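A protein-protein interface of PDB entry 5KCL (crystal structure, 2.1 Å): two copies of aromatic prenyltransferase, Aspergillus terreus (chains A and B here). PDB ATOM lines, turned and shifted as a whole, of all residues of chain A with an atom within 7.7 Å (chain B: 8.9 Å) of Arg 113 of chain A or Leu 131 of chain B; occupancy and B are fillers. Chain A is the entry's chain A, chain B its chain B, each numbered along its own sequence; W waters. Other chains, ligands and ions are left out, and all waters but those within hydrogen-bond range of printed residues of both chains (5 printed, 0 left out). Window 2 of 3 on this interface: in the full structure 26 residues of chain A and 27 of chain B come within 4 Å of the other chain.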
ATOM      1  N   LEU A 108     -20.197   3.797  11.326  1.00  0.00           N
ATOM      2  CA  LEU A 108     -21.235   2.732  11.463  1.00  0.00           C
ATOM      3  C   LEU A 108     -22.328   2.885  10.433  1.00  0.00           C
ATOM      4  O   LEU A 108     -23.358   2.213  10.490  1.00  0.00           O
ATOM      5  CB  LEU A 108     -21.826   2.831  12.883  1.00  0.00           C
ATOM      6  CG  LEU A 108     -20.804   2.484  13.975  1.00  0.00           C
ATOM      7  CD1 LEU A 108     -21.235   2.957  15.344  1.00  0.00           C
ATOM      8  CD2 LEU A 108     -20.643   1.000  14.012  1.00  0.00           C
ATOM      9  N   ALA A 109     -22.107   3.766   9.454  1.00  0.00           N
ATOM     10  CA  ALA A 109     -23.082   3.993   8.392  1.00  0.00           C
ATOM     11  C   ALA A 109     -23.492   2.717   7.715  1.00  0.00           C
ATOM     12  O   ALA A 109     -22.654   1.865   7.418  1.00  0.00           O
ATOM     13  CB  ALA A 109     -22.533   4.959   7.350  1.00  0.00           C
ATOM     14  N   GLY A 110     -24.794   2.604   7.447  1.00  0.00           N
ATOM     15  CA  GLY A 110     -25.344   1.472   6.678  1.00  0.00           C
ATOM     16  C   GLY A 110     -25.467   0.225   7.551  1.00  0.00           C
ATOM     17  O   GLY A 110     -25.629  -0.839   7.030  1.00  0.00           O
ATOM     18  N   THR A 111     -25.395   0.376   8.869  1.00  0.00           N
ATOM     19  CA  THR A 111     -25.566  -0.720   9.861  1.00  0.00           C
ATOM     20  C   THR A 111     -26.567  -0.290  10.887  1.00  0.00           C
ATOM     21  O   THR A 111     -27.040   0.853  10.856  1.00  0.00           O
ATOM     22  CB  THR A 111     -24.302  -1.056  10.605  1.00  0.00           C
ATOM     23  OG1 THR A 111     -24.011  -0.036  11.571  1.00  0.00           O
ATOM     24  CG2 THR A 111     -23.174  -1.224   9.659  1.00  0.00           C
ATOM     25  N   ALA A 112     -26.920  -1.188  11.792  1.00  0.00           N
ATOM     26  CA  ALA A 112     -28.075  -0.924  12.658  1.00  0.00           C
ATOM     27  C   ALA A 112     -27.947   0.325  13.549  1.00  0.00           C
ATOM     28  O   ALA A 112     -28.939   0.996  13.885  1.00  0.00           O
ATOM     29  CB  ALA A 112     -28.431  -2.173  13.508  1.00  0.00           C
ATOM     30  N   ARG A 113     -26.737   0.665  13.925  1.00  0.00           N
ATOM     31  CA  ARG A 113     -26.490   1.837  14.752  1.00  0.00           C
ATOM     32  C   ARG A 113     -26.567   3.172  13.982  1.00  0.00           C
ATOM     33  O   ARG A 113     -26.660   4.211  14.623  1.00  0.00           O
ATOM     34  CB  ARG A 113     -25.106   1.725  15.450  1.00  0.00           C
ATOM     35  CG  ARG A 113     -25.115   0.621  16.521  1.00  0.00           C
ATOM     36  CD  ARG A 113     -23.705   0.436  17.074  1.00  0.00           C
ATOM     37  NE  ARG A 113     -23.666  -0.657  18.025  1.00  0.00           N
ATOM     38  CZ  ARG A 113     -23.876  -0.545  19.335  1.00  0.00           C
ATOM     39  NH1 ARG A 113     -24.135   0.619  19.910  1.00  0.00           N
ATOM     40  NH2 ARG A 113     -23.876  -1.629  20.083  1.00  0.00           N
ATOM     41  N   ASP A 114     -26.622   3.133  12.645  1.00  0.00           N
ATOM     42  CA  ASP A 114     -26.709   4.331  11.821  1.00  0.00           C
ATOM     43  C   ASP A 114     -27.210   3.983  10.373  1.00  0.00           C
ATOM     44  O   ASP A 114     -26.425   4.054   9.415  1.00  0.00           O
ATOM     45  CB  ASP A 114     -25.315   4.977  11.813  1.00  0.00           C
ATOM     46  CG  ASP A 114     -25.252   6.280  11.040  1.00  0.00           C
ATOM     47  OD1 ASP A 114     -26.331   6.893  10.790  1.00  0.00           O
ATOM     48  OD2 ASP A 114     -24.109   6.744  10.721  1.00  0.00           O
ATOM     49  N   PRO A 115     -28.519   3.589  10.218  1.00  0.00           N
ATOM     50  CA  PRO A 115     -28.939   2.994   8.925  1.00  0.00           C
ATOM     51  C   PRO A 115     -28.920   3.965   7.732  1.00  0.00           C
ATOM     52  O   PRO A 115     -28.647   3.530   6.632  1.00  0.00           O
ATOM     53  CB  PRO A 115     -30.350   2.449   9.205  1.00  0.00           C
ATOM     54  CG  PRO A 115     -30.436   2.319  10.671  1.00  0.00           C
ATOM     55  CD  PRO A 115     -29.543   3.400  11.247  1.00  0.00           C
ATOM     56  N   LEU A 116     -29.125   5.267   7.968  1.00  0.00           N
ATOM     57  CA  LEU A 116     -29.169   6.255   6.897  1.00  0.00           C
ATOM     58  C   LEU A 116     -28.036   7.271   6.932  1.00  0.00           C
ATOM     59  O   LEU A 116     -28.150   8.387   6.364  1.00  0.00           O
ATOM     60  CB  LEU A 116     -30.499   7.001   6.941  1.00  0.00           C
ATOM     61  CG  LEU A 116     -31.798   6.242   6.653  1.00  0.00           C
ATOM     62  CD1 LEU A 116     -32.951   7.241   6.635  1.00  0.00           C
ATOM     63  CD2 LEU A 116     -31.777   5.545   5.324  1.00  0.00           C
ATOM     64  N   ASN A 117     -26.938   6.905   7.558  1.00  0.00           N
ATOM     65  CA  ASN A 117     -25.771   7.801   7.663  1.00  0.00           C
ATOM     66  C   ASN A 117     -26.164   9.207   8.133  1.00  0.00           C
ATOM     67  O   ASN A 117     -25.888  10.180   7.466  1.00  0.00           O
ATOM     68  CB  ASN A 117     -25.045   7.890   6.321  1.00  0.00           C
ATOM     69  CG  ASN A 117     -23.701   8.635   6.433  1.00  0.00           C
ATOM     70  OD1 ASN A 117     -22.862   8.320   7.295  1.00  0.00           O
ATOM     71  ND2 ASN A 117     -23.505   9.631   5.576  1.00  0.00           N
ATOM     72  N   SER A 118     -26.732   9.273   9.327  1.00  0.00           N
ATOM     73  CA  SER A 118     -27.326  10.482   9.869  1.00  0.00           C
ATOM     74  C   SER A 118     -26.401  11.456  10.556  1.00  0.00           C
ATOM     75  O   SER A 118     -26.877  12.497  10.914  1.00  0.00           O
ATOM     76  CB  SER A 118     -28.400  10.131  10.913  1.00  0.00           C
ATOM     77  OG  SER A 118     -29.501   9.505  10.274  1.00  0.00           O
ATOM     78  N   PHE A 119     -25.128  11.119  10.777  1.00  0.00           N
ATOM     79  CA  PHE A 119     -24.257  11.925  11.647  1.00  0.00           C
ATOM     80  C   PHE A 119     -22.965  12.454  10.992  1.00  0.00           C
ATOM     81  O   PHE A 119     -22.429  13.484  11.444  1.00  0.00           O
ATOM     82  CB  PHE A 119     -23.863  11.095  12.891  1.00  0.00           C
ATOM     83  CG  PHE A 119     -25.021  10.356  13.548  1.00  0.00           C
ATOM     84  CD1 PHE A 119     -26.023  11.053  14.204  1.00  0.00           C
ATOM     85  CD2 PHE A 119     -25.095   8.970  13.498  1.00  0.00           C
ATOM     86  CE1 PHE A 119     -27.145  10.421  14.761  1.00  0.00           C
ATOM     87  CE2 PHE A 119     -26.183   8.311  14.095  1.00  0.00           C
ATOM     88  CZ  PHE A 119     -27.208   9.032  14.711  1.00  0.00           C
ATOM     89  N   ARG A 151     -33.619   6.342  15.123  1.00  0.00           N
ATOM     90  CA  ARG A 151     -33.002   5.138  14.583  1.00  0.00           C
ATOM     91  C   ARG A 151     -34.050   4.167  14.048  1.00  0.00           C
ATOM     92  O   ARG A 151     -33.906   3.615  12.957  1.00  0.00           O
ATOM     93  CB  ARG A 151     -32.101   4.418  15.609  1.00  0.00           C
ATOM     94  CG  ARG A 151     -31.426   3.180  15.028  1.00  0.00           C
ATOM     95  CD  ARG A 151     -30.788   2.352  16.141  1.00  0.00           C
ATOM     96  NE  ARG A 151     -29.682   3.121  16.761  1.00  0.00           N
ATOM     97  CZ  ARG A 151     -28.818   2.631  17.664  1.00  0.00           C
ATOM     98  NH1 ARG A 151     -28.872   1.373  18.053  1.00  0.00           N
ATOM     99  NH2 ARG A 151     -27.892   3.423  18.193  1.00  0.00           N
ATOM    100  N   CYS A 154     -35.210   5.293  10.818  1.00  0.00           N
ATOM    101  CA  CYS A 154     -34.179   5.057   9.815  1.00  0.00           C
ATOM    102  C   CYS A 154     -34.212   3.588   9.337  1.00  0.00           C
ATOM    103  O   CYS A 154     -34.091   3.333   8.129  1.00  0.00           O
ATOM    104  CB  CYS A 154     -32.787   5.418  10.318  1.00  0.00           C
ATOM    105  SG  CYS A 154     -32.524   7.190  10.483  1.00  0.00           S
ATOM    106  N   LYS B  49     -21.719  -0.762  34.219  1.00  0.00           N
ATOM    107  CA  LYS B  49     -22.270  -0.151  33.008  1.00  0.00           C
ATOM    108  C   LYS B  49     -22.024   1.344  33.005  1.00  0.00           C
ATOM    109  O   LYS B  49     -21.535   1.917  31.999  1.00  0.00           O
ATOM    110  CB  LYS B  49     -23.766  -0.465  32.850  1.00  0.00           C
ATOM    111  CG  LYS B  49     -24.366   0.097  31.575  1.00  0.00           C
ATOM    112  CD  LYS B  49     -25.802  -0.294  31.387  1.00  0.00           C
ATOM    113  CE  LYS B  49     -26.355   0.339  30.106  1.00  0.00           C
ATOM    114  NZ  LYS B  49     -27.539  -0.468  29.642  1.00  0.00           N
ATOM    115  N   ALA B  52     -18.166   2.438  33.234  1.00  0.00           N
ATOM    116  CA  ALA B  52     -17.484   2.233  31.937  1.00  0.00           C
ATOM    117  C   ALA B  52     -17.901   3.281  30.884  1.00  0.00           C
ATOM    118  O   ALA B  52     -17.090   3.818  30.194  1.00  0.00           O
ATOM    119  CB  ALA B  52     -17.784   0.870  31.411  1.00  0.00           C
ATOM    120  N   PHE B  53     -19.204   3.560  30.837  1.00  0.00           N
ATOM    121  CA  PHE B  53     -19.766   4.653  30.077  1.00  0.00           C
ATOM    122  C   PHE B  53     -19.125   5.995  30.421  1.00  0.00           C
ATOM    123  O   PHE B  53     -18.803   6.795  29.531  1.00  0.00           O
ATOM    124  CB  PHE B  53     -21.309   4.701  30.293  1.00  0.00           C
ATOM    125  CG  PHE B  53     -21.930   5.916  29.799  1.00  0.00           C
ATOM    126  CD1 PHE B  53     -22.187   6.053  28.454  1.00  0.00           C
ATOM    127  CD2 PHE B  53     -22.203   6.961  30.639  1.00  0.00           C
ATOM    128  CE1 PHE B  53     -22.745   7.239  27.957  1.00  0.00           C
ATOM    129  CE2 PHE B  53     -22.777   8.154  30.149  1.00  0.00           C
ATOM    130  CZ  PHE B  53     -23.044   8.290  28.813  1.00  0.00           C
ATOM    131  N   TYR B  54     -19.032   6.273  31.718  1.00  0.00           N
ATOM    132  CA  TYR B  54     -18.470   7.523  32.210  1.00  0.00           C
ATOM    133  C   TYR B  54     -17.013   7.646  31.739  1.00  0.00           C
ATOM    134  O   TYR B  54     -16.604   8.706  31.250  1.00  0.00           O
ATOM    135  CB  TYR B  54     -18.545   7.542  33.728  1.00  0.00           C
ATOM    136  CG  TYR B  54     -17.990   8.775  34.417  1.00  0.00           C
ATOM    137  CD1 TYR B  54     -18.651   9.978  34.352  1.00  0.00           C
ATOM    138  CD2 TYR B  54     -16.861   8.708  35.190  1.00  0.00           C
ATOM    139  CE1 TYR B  54     -18.138  11.139  34.934  1.00  0.00           C
ATOM    140  CE2 TYR B  54     -16.346   9.857  35.807  1.00  0.00           C
ATOM    141  CZ  TYR B  54     -16.986  11.068  35.668  1.00  0.00           C
ATOM    142  OH  TYR B  54     -16.554  12.225  36.316  1.00  0.00           O
ATOM    143  N   LYS B  56     -15.473   6.147  29.043  1.00  0.00           N
ATOM    144  CA  LYS B  56     -15.337   6.182  27.587  1.00  0.00           C
ATOM    145  C   LYS B  56     -15.917   7.455  27.002  1.00  0.00           C
ATOM    146  O   LYS B  56     -15.291   8.016  26.160  1.00  0.00           O
ATOM    147  CB  LYS B  56     -16.099   5.018  26.966  1.00  0.00           C
ATOM    148  CG  LYS B  56     -16.207   5.006  25.421  1.00  0.00           C
ATOM    149  CD  LYS B  56     -14.862   4.865  24.725  1.00  0.00           C
ATOM    150  CE  LYS B  56     -15.023   5.256  23.231  1.00  0.00           C
ATOM    151  NZ  LYS B  56     -13.753   5.015  22.476  1.00  0.00           N
ATOM    152  N   TYR B  57     -17.087   7.913  27.483  1.00  0.00           N
ATOM    153  CA  TYR B  57     -17.806   9.026  26.886  1.00  0.00           C
ATOM    154  C   TYR B  57     -17.701  10.350  27.621  1.00  0.00           C
ATOM    155  O   TYR B  57     -17.727  11.415  26.989  1.00  0.00           O
ATOM    156  CB  TYR B  57     -19.323   8.673  26.724  1.00  0.00           C
ATOM    157  CG  TYR B  57     -19.478   7.629  25.669  1.00  0.00           C
ATOM    158  CD1 TYR B  57     -19.382   7.979  24.326  1.00  0.00           C
ATOM    159  CD2 TYR B  57     -19.554   6.282  25.997  1.00  0.00           C
ATOM    160  CE1 TYR B  57     -19.464   7.024  23.346  1.00  0.00           C
ATOM    161  CE2 TYR B  57     -19.626   5.316  25.019  1.00  0.00           C
ATOM    162  CZ  TYR B  57     -19.603   5.699  23.692  1.00  0.00           C
ATOM    163  OH  TYR B  57     -19.673   4.774  22.672  1.00  0.00           O
ATOM    164  N   ILE B  58     -17.614  10.312  28.942  1.00  0.00           N
ATOM    165  CA  ILE B  58     -17.700  11.534  29.692  1.00  0.00           C
ATOM    166  C   ILE B  58     -16.347  12.109  30.031  1.00  0.00           C
ATOM    167  O   ILE B  58     -16.161  13.329  29.870  1.00  0.00           O
ATOM    168  CB  ILE B  58     -18.563  11.386  30.970  1.00  0.00           C
ATOM    169  CG1 ILE B  58     -19.952  10.814  30.652  1.00  0.00           C
ATOM    170  CG2 ILE B  58     -18.657  12.742  31.703  1.00  0.00           C
ATOM    171  CD1 ILE B  58     -20.762  11.543  29.580  1.00  0.00           C
ATOM    172  N   LEU B 124     -20.790  15.056  21.837  1.00  0.00           N
ATOM    173  CA  LEU B 124     -21.151  14.029  22.796  1.00  0.00           C
ATOM    174  C   LEU B 124     -22.474  13.381  22.404  1.00  0.00           C
ATOM    175  O   LEU B 124     -22.610  12.176  22.443  1.00  0.00           O
ATOM    176  CB  LEU B 124     -21.287  14.620  24.218  1.00  0.00           C
ATOM    177  CG  LEU B 124     -21.821  13.696  25.308  1.00  0.00           C
ATOM    178  CD1 LEU B 124     -20.925  12.456  25.444  1.00  0.00           C
ATOM    179  CD2 LEU B 124     -21.823  14.421  26.639  1.00  0.00           C
ATOM    180  N   LEU B 125     -23.468  14.164  22.055  1.00  0.00           N
ATOM    181  CA  LEU B 125     -24.791  13.584  21.777  1.00  0.00           C
ATOM    182  C   LEU B 125     -24.817  12.694  20.547  1.00  0.00           C
ATOM    183  O   LEU B 125     -25.522  11.690  20.524  1.00  0.00           O
ATOM    184  CB  LEU B 125     -25.825  14.682  21.642  1.00  0.00           C
ATOM    185  CG  LEU B 125     -26.205  15.192  23.036  1.00  0.00           C
ATOM    186  CD1 LEU B 125     -26.602  16.644  22.986  1.00  0.00           C
ATOM    187  CD2 LEU B 125     -27.354  14.323  23.543  1.00  0.00           C
ATOM    188  N   LYS B 126     -24.024  13.046  19.556  1.00  0.00           N
ATOM    189  CA  LYS B 126     -23.849  12.241  18.370  1.00  0.00           C
ATOM    190  C   LYS B 126     -23.263  10.853  18.748  1.00  0.00           C
ATOM    191  O   LYS B 126     -23.821   9.850  18.365  1.00  0.00           O
ATOM    192  CB  LYS B 126     -22.930  12.942  17.379  1.00  0.00           C
ATOM    193  CG  LYS B 126     -22.466  12.055  16.257  1.00  0.00           C
ATOM    194  CD  LYS B 126     -21.068  12.396  15.773  1.00  0.00           C
ATOM    195  CE  LYS B 126     -20.010  11.774  16.641  1.00  0.00           C
ATOM    196  NZ  LYS B 126     -18.654  12.370  16.364  1.00  0.00           N
ATOM    197  N   ASN B 127     -22.210  10.828  19.552  1.00  0.00           N
ATOM    198  CA  ASN B 127     -21.682   9.555  20.119  1.00  0.00           C
ATOM    199  C   ASN B 127     -22.709   8.772  20.921  1.00  0.00           C
ATOM    200  O   ASN B 127     -22.825   7.596  20.750  1.00  0.00           O
ATOM    201  CB  ASN B 127     -20.449   9.823  20.934  1.00  0.00           C
ATOM    202  CG  ASN B 127     -19.309  10.266  20.057  1.00  0.00           C
ATOM    203  OD1 ASN B 127     -19.289   9.938  18.885  1.00  0.00           O
ATOM    204  ND2 ASN B 127     -18.482  11.126  20.550  1.00  0.00           N
ATOM    205  N   LEU B 128     -23.489   9.433  21.734  1.00  0.00           N
ATOM    206  CA  LEU B 128     -24.598   8.839  22.415  1.00  0.00           C
ATOM    207  C   LEU B 128     -25.672   8.254  21.466  1.00  0.00           C
ATOM    208  O   LEU B 128     -26.269   7.222  21.779  1.00  0.00           O
ATOM    209  CB  LEU B 128     -25.218   9.825  23.417  1.00  0.00           C
ATOM    210  CG  LEU B 128     -24.329  10.363  24.563  1.00  0.00           C
ATOM    211  CD1 LEU B 128     -25.180  11.113  25.575  1.00  0.00           C
ATOM    212  CD2 LEU B 128     -23.468   9.302  25.276  1.00  0.00           C
ATOM    213  N   ALA B 129     -25.881   8.861  20.300  1.00  0.00           N
ATOM    214  CA  ALA B 129     -26.918   8.375  19.373  1.00  0.00           C
ATOM    215  C   ALA B 129     -26.531   7.106  18.638  1.00  0.00           C
ATOM    216  O   ALA B 129     -27.408   6.345  18.277  1.00  0.00           O
ATOM    217  CB  ALA B 129     -27.279   9.428  18.338  1.00  0.00           C
ATOM    218  N   THR B 130     -25.235   6.865  18.414  1.00  0.00           N
ATOM    219  CA  THR B 130     -24.811   5.571  17.930  1.00  0.00           C
ATOM    220  C   THR B 130     -24.665   4.556  19.064  1.00  0.00           C
ATOM    221  O   THR B 130     -24.637   3.355  18.813  1.00  0.00           O
ATOM    222  CB  THR B 130     -23.519   5.658  17.061  1.00  0.00           C
ATOM    223  OG1 THR B 130     -22.451   6.165  17.832  1.00  0.00           O
ATOM    224  CG2 THR B 130     -23.739   6.572  15.901  1.00  0.00           C
ATOM    225  N   LEU B 131     -24.502   5.008  20.308  1.00  0.00           N
ATOM    226  CA  LEU B 131     -24.443   4.114  21.450  1.00  0.00           C
ATOM    227  C   LEU B 131     -25.805   3.619  21.867  1.00  0.00           C
ATOM    228  O   LEU B 131     -25.977   2.430  22.121  1.00  0.00           O
ATOM    229  CB  LEU B 131     -23.877   4.815  22.661  1.00  0.00           C
ATOM    230  CG  LEU B 131     -23.804   4.001  23.939  1.00  0.00           C
ATOM    231  CD1 LEU B 131     -22.789   2.895  23.754  1.00  0.00           C
ATOM    232  CD2 LEU B 131     -23.392   4.937  25.074  1.00  0.00           C
ATOM    233  N   LEU B 132     -26.765   4.529  21.943  1.00  0.00           N
ATOM    234  CA  LEU B 132     -28.059   4.296  22.606  1.00  0.00           C
ATOM    235  C   LEU B 132     -29.223   4.333  21.578  1.00  0.00           C
ATOM    236  O   LEU B 132     -29.466   5.381  20.954  1.00  0.00           O
ATOM    237  CB  LEU B 132     -28.278   5.409  23.626  1.00  0.00           C
ATOM    238  CG  LEU B 132     -27.221   5.678  24.714  1.00  0.00           C
ATOM    239  CD1 LEU B 132     -27.392   7.051  25.355  1.00  0.00           C
ATOM    240  CD2 LEU B 132     -27.251   4.648  25.791  1.00  0.00           C
ATOM    241  N   PRO B 133     -30.017   3.251  21.458  1.00  0.00           N
ATOM    242  CA  PRO B 133     -31.131   3.194  20.453  1.00  0.00           C
ATOM    243  C   PRO B 133     -32.265   4.229  20.604  1.00  0.00           C
ATOM    244  O   PRO B 133     -32.926   4.551  19.634  1.00  0.00           O
ATOM    245  CB  PRO B 133     -31.721   1.781  20.685  1.00  0.00           C
ATOM    246  CG  PRO B 133     -31.512   1.555  22.133  1.00  0.00           C
ATOM    247  CD  PRO B 133     -30.158   2.183  22.475  1.00  0.00           C
ATOM    248  N   HIS B 134     -32.498   4.711  21.817  1.00  0.00           N
ATOM    249  CA  HIS B 134     -33.591   5.613  22.151  1.00  0.00           C
ATOM    250  C   HIS B 134     -33.209   7.113  22.192  1.00  0.00           C
ATOM    251  O   HIS B 134     -34.034   7.955  22.560  1.00  0.00           O
ATOM    252  CB  HIS B 134     -34.088   5.247  23.553  1.00  0.00           C
ATOM    253  CG  HIS B 134     -33.039   5.499  24.624  1.00  0.00           C
ATOM    254  ND1 HIS B 134     -31.979   4.635  24.873  1.00  0.00           N
ATOM    255  CD2 HIS B 134     -32.835   6.575  25.436  1.00  0.00           C
ATOM    256  CE1 HIS B 134     -31.234   5.131  25.850  1.00  0.00           C
ATOM    257  NE2 HIS B 134     -31.716   6.316  26.195  1.00  0.00           N
ATOM    258  N   VAL B 135     -31.976   7.468  21.887  1.00  0.00           N
ATOM    259  CA  VAL B 135     -31.563   8.872  21.900  1.00  0.00           C
ATOM    260  C   VAL B 135     -32.059   9.535  20.634  1.00  0.00           C
ATOM    261  O   VAL B 135     -32.023   8.951  19.583  1.00  0.00           O
ATOM    262  CB  VAL B 135     -30.028   8.999  22.016  1.00  0.00           C
ATOM    263  CG1 VAL B 135     -29.563  10.418  21.735  1.00  0.00           C
ATOM    264  CG2 VAL B 135     -29.654   8.637  23.420  1.00  0.00           C
ATOM    265  N   LEU B 173     -27.413  13.659  32.237  1.00  0.00           N
ATOM    266  CA  LEU B 173     -27.619  12.247  31.899  1.00  0.00           C
ATOM    267  C   LEU B 173     -28.269  11.616  33.124  1.00  0.00           C
ATOM    268  O   LEU B 173     -27.634  11.505  34.176  1.00  0.00           O
ATOM    269  CB  LEU B 173     -26.262  11.634  31.609  1.00  0.00           C
ATOM    270  CG  LEU B 173     -25.511  12.380  30.484  1.00  0.00           C
ATOM    271  CD1 LEU B 173     -24.071  11.910  30.385  1.00  0.00           C
ATOM    272  CD2 LEU B 173     -26.202  12.119  29.173  1.00  0.00           C
ATOM    273  N   GLU B 179     -30.581   2.512  31.835  1.00  0.00           N
ATOM    274  CA  GLU B 179     -30.314   3.244  30.630  1.00  0.00           C
ATOM    275  C   GLU B 179     -29.638   4.561  30.997  1.00  0.00           C
ATOM    276  O   GLU B 179     -29.567   4.925  32.194  1.00  0.00           O
ATOM    277  CB  GLU B 179     -31.655   3.503  29.897  1.00  0.00           C
ATOM    278  CG  GLU B 179     -32.138   2.302  29.105  1.00  0.00           C
ATOM    279  CD  GLU B 179     -31.197   1.955  27.942  1.00  0.00           C
ATOM    280  OE1 GLU B 179     -30.225   2.735  27.643  1.00  0.00           O
ATOM    281  OE2 GLU B 179     -31.436   0.899  27.314  1.00  0.00           O
ATOM    282  N   VAL B 180     -29.212   5.280  29.969  1.00  0.00           N
ATOM    283  CA  VAL B 180     -28.676   6.637  30.108  1.00  0.00           C
ATOM    284  C   VAL B 180     -29.638   7.464  29.335  1.00  0.00           C
ATOM    285  O   VAL B 180     -29.875   7.182  28.150  1.00  0.00           O
ATOM    286  CB  VAL B 180     -27.275   6.764  29.459  1.00  0.00           C
ATOM    287  CG1 VAL B 180     -26.821   8.217  29.425  1.00  0.00           C
ATOM    288  CG2 VAL B 180     -26.314   5.888  30.213  1.00  0.00           C
ATOM    289  N   PRO B 182     -30.518  11.286  28.093  1.00  0.00           N
ATOM    290  CA  PRO B 182     -29.950  12.620  28.055  1.00  0.00           C
ATOM    291  C   PRO B 182     -31.009  13.673  28.031  1.00  0.00           C
ATOM    292  O   PRO B 182     -32.059  13.449  27.444  1.00  0.00           O
ATOM    293  CB  PRO B 182     -29.179  12.683  26.725  1.00  0.00           C
ATOM    294  CG  PRO B 182     -29.156  11.346  26.194  1.00  0.00           C
ATOM    295  CD  PRO B 182     -30.212  10.543  26.864  1.00  0.00           C
HETATM  296  O   HOH W   1     -35.079   4.872  17.488  1.00  0.00           O
HETATM  297  O   HOH W   2     -33.073   6.917  17.998  1.00  0.00           O
HETATM  298  O   HOH W   3     -27.255   0.854  20.374  1.00  0.00           O
HETATM  299  O   HOH W   4     -28.541   5.692  15.571  1.00  0.00           O
HETATM  300  O   HOH W   5     -24.313  -0.616  22.506  1.00  0.00           O
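O of Thr 130 of chain B lies within hydrogen-bond range of NH1 of Arg 113 of chain A (3.0 Å). The guanidinium group of Arg 151 of chain A sits at hydrogen-bond distance from the backbone carbonyl oxygen of Thr 130 of chain B (3.3 Å). NH1 of Arg 113 of chain A lies within hydrogen-bond range of O of Leu 131 of chain B, at 3.4 Å. NH2 of Arg 151 of chain A lies within hydrogen-bond range of O of Ala 129 of chain B, 3.0 Å away.
O of Asn 127 of chain B sits at hydrogen-bond distance from OG1 of Thr 130 of chain B (3.3 Å). The side-chain hydroxyl (OG1) of Thr 111 of chain A lies within hydrogen-bond range of the backbone carbonyl oxygen (O) of Leu 108 of chain A (2.6 Å).
Of the printed residues of chain B, Leu 108 of chain A touches Thr 130. Of chain B, only Thr 130 and Leu 131 come within 4 Å of Arg 113 of chain A. Of the printed residues of chain B, Phe 119 of chain A touches Lys 126, Ala 129 and Thr 130. Printed residues of chain A within 4 Å of Lys 126 of chain B: Phe 119 (3.8 Å). Of the printed residues of chain A, Thr 130 of chain B touches Leu 108, Arg 113, Phe 119 and Arg 151. Leu 131 of chain B touches just one residue of chain A: Arg 113 (3.4 Å). The nearest residue of chain B that does not touch Arg 113 of chain A is Ala 129 of chain B (4.3 Å). The nearest residue of chain A that does not touch Leu 131 of chain B is Arg 151 of chain A (4.2 Å).
No position is printed for both chains.
Of the 14 printed residues of chain A, 4 touch a printed residue of chain B. Of the 23 printed residues of chain B, 6 touch a printed residue of chain A. Among the printed residues, no Asp or Glu carboxylate lies within 4 Å of a Lys or Arg side-chain nitrogen of the other chain.
Among the printed residues, pairs that only touch across the chains: Phe 119 of chain A with Thr 130 of chain B (3.5 Å), Phe 119 of chain A with Ala 129 of chain B (3.6 Å), Arg 151 of chain A with Pro 133 of chain B (3.7 Å), Arg 151 of chain A with Leu 132 of chain B (3.7 Å), Phe 119 of chain A with Lys 126 of chain B (3.8 Å) and Leu 108 of chain A with Thr 130 of chain B (3.9 Å).
Water W4 lies within hydrogen-bond range of the backbone carbonyl oxygen (O) of Arg 113 of chain A (2.6 Å), the backbone carbonyl oxygen (O) of Ala 129 of chain B (3.0 Å) and the guanidinium group (NE) of Arg 151 of chain A (3.1 Å). Water W5 bridges the guanidinium group (NH2) of Arg 113 of chain A (2.7 Å) and the backbone carbonyl oxygen (O) of Leu 131 of chain B (3.5 Å). Water W3 lies within hydrogen-bond range of O of Leu 131 of chain B (2.7 Å), NH1 of Arg 151 of chain A (2.9 Å) and NH1 of Arg 113 of chain A (3.2 Å). Water W2 lies within hydrogen-bond range of O of Val 135 of chain B (2.8 Å), O of Pro 133 of chain B (2.9 Å) and N of Arg 151 of chain A (3.0 Å). Water W1 bridges the backbone carbonyl oxygen (O) of Pro 133 of chain B and the backbone NH (N) of Arg 151 of chain A.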
